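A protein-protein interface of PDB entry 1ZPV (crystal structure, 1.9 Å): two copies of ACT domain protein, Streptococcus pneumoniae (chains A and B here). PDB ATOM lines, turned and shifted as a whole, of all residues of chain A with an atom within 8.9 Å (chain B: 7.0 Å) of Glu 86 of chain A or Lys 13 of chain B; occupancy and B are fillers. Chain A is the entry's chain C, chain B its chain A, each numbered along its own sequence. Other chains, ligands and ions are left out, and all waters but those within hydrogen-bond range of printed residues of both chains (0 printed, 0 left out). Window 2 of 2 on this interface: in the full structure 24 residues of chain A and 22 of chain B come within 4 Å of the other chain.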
ATOM      1  N   LYS A   5      12.269   6.072  -2.060  1.00  0.00           N
ATOM      2  CA  LYS A   5      12.427   4.636  -1.788  1.00  0.00           C
ATOM      3  C   LYS A   5      11.046   4.076  -1.550  1.00  0.00           C
ATOM      4  O   LYS A   5      10.203   4.760  -0.950  1.00  0.00           O
ATOM      5  CB  LYS A   5      13.297   4.395  -0.551  1.00  0.00           C
ATOM      6  CG  LYS A   5      13.803   2.965  -0.398  1.00  0.00           C
ATOM      7  CD  LYS A   5      15.055   2.882   0.498  1.00  0.00           C
ATOM      8  CE  LYS A   5      16.362   3.065  -0.283  1.00  0.00           C
ATOM      9  NZ  LYS A   5      16.589   2.030  -1.368  1.00  0.00           N
ATOM     10  N   ILE A   7       8.571   0.040  -1.330  1.00  0.00           N
ATOM     11  CA  ILE A   7       8.494  -1.414  -1.283  1.00  0.00           C
ATOM     12  C   ILE A   7       7.323  -1.823  -2.170  1.00  0.00           C
ATOM     13  O   ILE A   7       6.225  -1.323  -1.996  1.00  0.00           O
ATOM     14  CB  ILE A   7       8.287  -1.937   0.171  1.00  0.00           C
ATOM     15  CG1 ILE A   7       9.449  -1.478   1.091  1.00  0.00           C
ATOM     16  CG2 ILE A   7       8.223  -3.459   0.172  1.00  0.00           C
ATOM     17  CD1 ILE A   7       9.237  -0.093   1.718  1.00  0.00           C
ATOM     18  N   SER A  81       5.513   3.918  -0.195  1.00  0.00           N
ATOM     19  CA  SER A  81       6.697   4.752   0.052  1.00  0.00           C
ATOM     20  C   SER A  81       7.303   4.322   1.379  1.00  0.00           C
ATOM     21  O   SER A  81       6.572   4.138   2.378  1.00  0.00           O
ATOM     22  CB  SER A  81       6.318   6.244   0.130  1.00  0.00           C
ATOM     23  OG  SER A  81       7.461   6.992   0.435  1.00  0.00           O
ATOM     24  N   ALA A  82       8.630   4.250   1.416  1.00  0.00           N
ATOM     25  CA  ALA A  82       9.388   3.965   2.642  1.00  0.00           C
ATOM     26  C   ALA A  82       9.319   5.118   3.667  1.00  0.00           C
ATOM     27  O   ALA A  82       9.583   4.909   4.854  1.00  0.00           O
ATOM     28  CB  ALA A  82      10.841   3.682   2.285  1.00  0.00           C
ATOM     29  N   ALA A  83       8.942   6.315   3.207  1.00  0.00           N
ATOM     30  CA  ALA A  83       8.842   7.502   4.080  1.00  0.00           C
ATOM     31  C   ALA A  83       7.973   7.255   5.307  1.00  0.00           C
ATOM     32  O   ALA A  83       8.199   7.839   6.380  1.00  0.00           O
ATOM     33  CB  ALA A  83       8.333   8.728   3.299  1.00  0.00           C
ATOM     34  N   ILE A  84       6.950   6.417   5.137  1.00  0.00           N
ATOM     35  CA  ILE A  84       6.037   6.130   6.227  1.00  0.00           C
ATOM     36  C   ILE A  84       6.733   5.495   7.456  1.00  0.00           C
ATOM     37  O   ILE A  84       6.359   5.787   8.609  1.00  0.00           O
ATOM     38  CB  ILE A  84       4.847   5.267   5.726  1.00  0.00           C
ATOM     39  CG1 ILE A  84       4.047   6.040   4.666  1.00  0.00           C
ATOM     40  CG2 ILE A  84       3.938   4.851   6.872  1.00  0.00           C
ATOM     41  CD1 ILE A  84       3.719   7.486   5.055  1.00  0.00           C
ATOM     42  N   PHE A  85       7.780   4.700   7.211  1.00  0.00           N
ATOM     43  CA  PHE A  85       8.567   4.069   8.275  1.00  0.00           C
ATOM     44  C   PHE A  85       9.707   4.943   8.832  1.00  0.00           C
ATOM     45  O   PHE A  85      10.382   4.554   9.775  1.00  0.00           O
ATOM     46  CB  PHE A  85       9.132   2.730   7.786  1.00  0.00           C
ATOM     47  CG  PHE A  85       8.118   1.872   7.083  1.00  0.00           C
ATOM     48  CD1 PHE A  85       7.113   1.227   7.813  1.00  0.00           C
ATOM     49  CD2 PHE A  85       8.149   1.719   5.707  1.00  0.00           C
ATOM     50  CE1 PHE A  85       6.167   0.440   7.160  1.00  0.00           C
ATOM     51  CE2 PHE A  85       7.205   0.939   5.046  1.00  0.00           C
ATOM     52  CZ  PHE A  85       6.217   0.303   5.774  1.00  0.00           C
ATOM     53  N   GLU A  86       9.909   6.123   8.257  1.00  0.00           N
ATOM     54  CA  GLU A  86      11.067   6.976   8.609  1.00  0.00           C
ATOM     55  C   GLU A  86      10.624   8.276   9.252  1.00  0.00           C
ATOM     56  O   GLU A  86      11.262   8.765  10.202  1.00  0.00           O
ATOM     57  CB  GLU A  86      11.910   7.338   7.367  1.00  0.00           C
ATOM     58  CG  GLU A  86      12.341   6.191   6.461  1.00  0.00           C
ATOM     59  CD  GLU A  86      13.513   5.365   6.992  1.00  0.00           C
ATOM     60  OE1 GLU A  86      14.221   5.821   7.917  1.00  0.00           O
ATOM     61  OE2 GLU A  86      13.733   4.252   6.462  1.00  0.00           O
ATOM     62  N   ALA A  87       9.537   8.841   8.722  1.00  0.00           N
ATOM     63  CA  ALA A  87       9.205  10.239   8.964  1.00  0.00           C
ATOM     64  C   ALA A  87       8.773  10.473  10.403  1.00  0.00           C
ATOM     65  O   ALA A  87       8.197   9.586  11.037  1.00  0.00           O
ATOM     66  CB  ALA A  87       8.140  10.730   7.994  1.00  0.00           C
ATOM     67  N   MET A  88       9.052  11.678  10.894  1.00  0.00           N
ATOM     68  CA  MET A  88       8.625  12.089  12.220  1.00  0.00           C
ATOM     69  C   MET A  88       7.205  12.639  12.165  1.00  0.00           C
ATOM     70  O   MET A  88       6.790  13.141  11.113  1.00  0.00           O
ATOM     71  CB  MET A  88       9.569  13.170  12.774  1.00  0.00           C
ATOM     72  CG  MET A  88      11.013  12.731  12.914  1.00  0.00           C
ATOM     73  SD  MET A  88      12.099  14.083  13.830  1.00  0.00           S
ATOM     74  CE  MET A  88      11.732  15.619  12.660  1.00  0.00           C
ATOM     75  N   TYR A  89       6.468  12.523  13.279  1.00  0.00           N
ATOM     76  CA  TYR A  89       5.188  13.248  13.508  1.00  0.00           C
ATOM     77  C   TYR A  89       4.902  13.437  15.004  1.00  0.00           C
ATOM     78  O   TYR A  89       3.822  13.106  15.506  1.00  0.00           O
ATOM     79  CB  TYR A  89       3.983  12.606  12.784  1.00  0.00           C
ATOM     80  CG  TYR A  89       4.040  12.727  11.265  1.00  0.00           C
ATOM     81  CD1 TYR A  89       4.220  11.595  10.459  1.00  0.00           C
ATOM     82  CD2 TYR A  89       3.952  13.974  10.639  1.00  0.00           C
ATOM     83  CE1 TYR A  89       4.304  11.702   9.076  1.00  0.00           C
ATOM     84  CE2 TYR A  89       4.032  14.087   9.245  1.00  0.00           C
ATOM     85  CZ  TYR A  89       4.209  12.948   8.476  1.00  0.00           C
ATOM     86  OH  TYR A  89       4.282  13.059   7.098  1.00  0.00           O
ATOM     87  N   VAL B  11       4.772  -5.130   6.080  1.00  0.00           N
ATOM     88  CA  VAL B  11       6.005  -4.428   5.704  1.00  0.00           C
ATOM     89  C   VAL B  11       6.384  -3.518   6.850  1.00  0.00           C
ATOM     90  O   VAL B  11       5.556  -2.757   7.373  1.00  0.00           O
ATOM     91  CB  VAL B  11       5.854  -3.617   4.392  1.00  0.00           C
ATOM     92  CG1 VAL B  11       7.209  -3.058   3.947  1.00  0.00           C
ATOM     93  CG2 VAL B  11       5.200  -4.484   3.235  1.00  0.00           C
ATOM     94  N   GLY B  12       7.644  -3.597   7.263  1.00  0.00           N
ATOM     95  CA  GLY B  12       8.108  -2.737   8.322  1.00  0.00           C
ATOM     96  C   GLY B  12       9.606  -2.616   8.267  1.00  0.00           C
ATOM     97  O   GLY B  12      10.219  -3.133   7.354  1.00  0.00           O
ATOM     98  N   LYS B  13      10.188  -1.938   9.241  1.00  0.00           N
ATOM     99  CA  LYS B  13      11.630  -1.816   9.310  1.00  0.00           C
ATOM    100  C   LYS B  13      12.292  -2.766  10.291  1.00  0.00           C
ATOM    101  O   LYS B  13      13.426  -3.213  10.050  1.00  0.00           O
ATOM    102  CB  LYS B  13      12.023  -0.381   9.674  1.00  0.00           C
ATOM    103  CG  LYS B  13      11.915   0.564   8.525  1.00  0.00           C
ATOM    104  CD  LYS B  13      12.590   1.873   8.857  1.00  0.00           C
ATOM    105  CE  LYS B  13      14.084   1.740   8.799  1.00  0.00           C
ATOM    106  NZ  LYS B  13      14.688   3.093   8.910  1.00  0.00           N
ATOM    107  N   ASP B  14      11.624  -3.033  11.412  1.00  0.00           N
ATOM    108  CA  ASP B  14      12.170  -3.941  12.431  1.00  0.00           C
ATOM    109  C   ASP B  14      11.433  -5.270  12.407  1.00  0.00           C
ATOM    110  O   ASP B  14      10.219  -5.283  12.404  1.00  0.00           O
ATOM    111  CB  ASP B  14      12.071  -3.319  13.831  1.00  0.00           C
ATOM    112  CG  ASP B  14      13.007  -3.978  14.824  1.00  0.00           C
ATOM    113  OD1 ASP B  14      13.046  -5.228  14.880  1.00  0.00           O
ATOM    114  OD2 ASP B  14      13.714  -3.247  15.560  1.00  0.00           O
ATOM    115  N   LYS B  15      12.175  -6.376  12.383  1.00  0.00           N
ATOM    116  CA  LYS B  15      11.578  -7.719  12.410  1.00  0.00           C
ATOM    117  C   LYS B  15      11.121  -8.129  13.793  1.00  0.00           C
ATOM    118  O   LYS B  15      10.312  -9.052  13.928  1.00  0.00           O
ATOM    119  CB  LYS B  15      12.549  -8.797  11.863  1.00  0.00           C
ATOM    120  CG  LYS B  15      13.779  -9.130  12.714  1.00  0.00           C
ATOM    121  CD  LYS B  15      15.062  -8.402  12.264  1.00  0.00           C
ATOM    122  CE  LYS B  15      15.217  -6.986  12.858  1.00  0.00           C
ATOM    123  NZ  LYS B  15      15.565  -6.971  14.318  1.00  0.00           N
ATOM    124  N   SER B  16      11.661  -7.452  14.815  1.00  0.00           N
ATOM    125  CA  SER B  16      11.523  -7.903  16.196  1.00  0.00           C
ATOM    126  C   SER B  16      10.066  -8.072  16.645  1.00  0.00           C
ATOM    127  O   SER B  16       9.272  -7.142  16.578  1.00  0.00           O
ATOM    128  CB  SER B  16      12.268  -6.985  17.168  1.00  0.00           C
ATOM    129  OG  SER B  16      12.356  -7.625  18.425  1.00  0.00           O
ATOM    130  N   GLU B  43      16.585  -2.680   3.866  1.00  0.00           N
ATOM    131  CA  GLU B  43      16.570  -2.309   5.277  1.00  0.00           C
ATOM    132  C   GLU B  43      15.239  -2.692   5.968  1.00  0.00           C
ATOM    133  O   GLU B  43      14.966  -2.283   7.105  1.00  0.00           O
ATOM    134  CB  GLU B  43      16.804  -0.796   5.416  1.00  0.00           C
ATOM    135  CG  GLU B  43      18.237  -0.398   5.075  1.00  0.00           C
ATOM    136  CD  GLU B  43      19.256  -1.043   6.032  1.00  0.00           C
ATOM    137  OE1 GLU B  43      19.004  -1.044   7.271  1.00  0.00           O
ATOM    138  OE2 GLU B  43      20.290  -1.557   5.546  1.00  0.00           O
ATOM    139  N   TYR B  44      14.430  -3.478   5.271  1.00  0.00           N
ATOM    140  CA  TYR B  44      13.056  -3.803   5.723  1.00  0.00           C
ATOM    141  C   TYR B  44      12.892  -5.293   6.021  1.00  0.00           C
ATOM    142  O   TYR B  44      13.573  -6.115   5.425  1.00  0.00           O
ATOM    143  CB  TYR B  44      12.035  -3.296   4.678  1.00  0.00           C
ATOM    144  CG  TYR B  44      12.299  -1.851   4.371  1.00  0.00           C
ATOM    145  CD1 TYR B  44      11.794  -0.834   5.192  1.00  0.00           C
ATOM    146  CD2 TYR B  44      13.113  -1.494   3.304  1.00  0.00           C
ATOM    147  CE1 TYR B  44      12.089   0.500   4.940  1.00  0.00           C
ATOM    148  CE2 TYR B  44      13.417  -0.169   3.041  1.00  0.00           C
ATOM    149  CZ  TYR B  44      12.897   0.817   3.858  1.00  0.00           C
ATOM    150  OH  TYR B  44      13.217   2.101   3.586  1.00  0.00           O
ATOM    151  N   PHE B  45      12.043  -5.623   7.019  1.00  0.00           N
ATOM    152  CA  PHE B  45      11.596  -7.006   7.308  1.00  0.00           C
ATOM    153  C   PHE B  45      10.228  -7.125   6.754  1.00  0.00           C
ATOM    154  O   PHE B  45       9.389  -6.245   6.996  1.00  0.00           O
ATOM    155  CB  PHE B  45      11.477  -7.267   8.817  1.00  0.00           C
ATOM    156  CG  PHE B  45      10.940  -8.661   9.164  1.00  0.00           C
ATOM    157  CD1 PHE B  45      11.724  -9.808   8.948  1.00  0.00           C
ATOM    158  CD2 PHE B  45       9.666  -8.822   9.725  1.00  0.00           C
ATOM    159  CE1 PHE B  45      11.249 -11.091   9.277  1.00  0.00           C
ATOM    160  CE2 PHE B  45       9.171 -10.117  10.051  1.00  0.00           C
ATOM    161  CZ  PHE B  45       9.965 -11.244   9.817  1.00  0.00           C
ATOM    162  N   ASN B  74       4.364  -0.736  14.571  1.00  0.00           N
ATOM    163  CA  ASN B  74       5.077   0.093  13.623  1.00  0.00           C
ATOM    164  C   ASN B  74       5.263  -0.563  12.263  1.00  0.00           C
ATOM    165  O   ASN B  74       6.301  -0.415  11.648  1.00  0.00           O
ATOM    166  CB  ASN B  74       6.404   0.600  14.217  1.00  0.00           C
ATOM    167  CG  ASN B  74       6.180   1.497  15.404  1.00  0.00           C
ATOM    168  OD1 ASN B  74       5.397   2.451  15.335  1.00  0.00           O
ATOM    169  ND2 ASN B  74       6.841   1.187  16.519  1.00  0.00           N
ATOM    170  N   VAL B  75       4.233  -1.269  11.782  1.00  0.00           N
ATOM    171  CA  VAL B  75       4.323  -1.942  10.492  1.00  0.00           C
ATOM    172  C   VAL B  75       3.033  -1.700   9.706  1.00  0.00           C
ATOM    173  O   VAL B  75       1.995  -1.369  10.276  1.00  0.00           O
ATOM    174  CB  VAL B  75       4.576  -3.463  10.641  1.00  0.00           C
ATOM    175  CG1 VAL B  75       5.883  -3.744  11.402  1.00  0.00           C
ATOM    176  CG2 VAL B  75       3.366  -4.182  11.336  1.00  0.00           C
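Of chain B, only Lys 13 (2.9 Å) and Tyr 44 (3.6 Å) come within 4 Å of Glu 86 of chain A.
Of chain A, only Phe 85 (3.6 Å) and Glu 86 (2.9 Å) come within 4 Å of Lys 13 of chain B.
Of the printed residues of chain B, Ala 82 of chain A touches Tyr 44 (3.1 Å).
Of the printed residues of chain A, Tyr 44 of chain B touches Lys 5, Ala 82 and Glu 86.
The nearest residue of chain B that does not touch Glu 86 of chain A is Glu 43 of chain B (6.0 Å).
No position is printed for both chains.
O of Gly 12 of chain B sits at hydrogen-bond distance from N of Phe 45 of chain B (3.1 Å).
N of Ala 82 of chain A is in hydrogen-bond range of O of Lys 5 of chain A, 2.9 Å away.
Lys 5 of chain A touches Tyr 44 of chain B.
Val 11 of chain B touches Ile 7 of chain A.
Ala 82 of chain A touches Tyr 44 of chain B.
O of Val 11 of chain B touches CE1 of Phe 85 of chain A, 3.3 Å away.
Phe 85 of chain A touches Gly 12 of chain B.
Lys 13 of chain B touches Phe 85 of chain A.
Glu 86 of chain A touches Tyr 44 of chain B.
Of the 11 printed residues of chain B, 4 touch a printed residue of chain A.
Printed residues of chain B that touch a printed residue of chain A: Val 11, Gly 12, Lys 13 and Tyr 44.
Hydrophobic or aromatic side chains of chain B within 4 Å of the printed part of chain A: Val 11 and Tyr 44.
Along chain B the printed residues that touch a printed residue of chain A span positions 11 to 44.
Of the 11 printed residues of chain A, 5 touch a printed residue of chain B.
Printed residues of chain A that touch a printed residue of chain B: Lys 5, Ile 7, Ala 82, Phe 85 and Glu 86.
Hydrophobic or aromatic side chains of chain A that line the printed part of chain B: Ile 7, Ala 82 and Phe 85.
Among the printed residues, 8 pairs touch across the chains.
NZ of Lys 13 of chain B lies within salt-bridge range of OE2 of Glu 86 of chain A.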
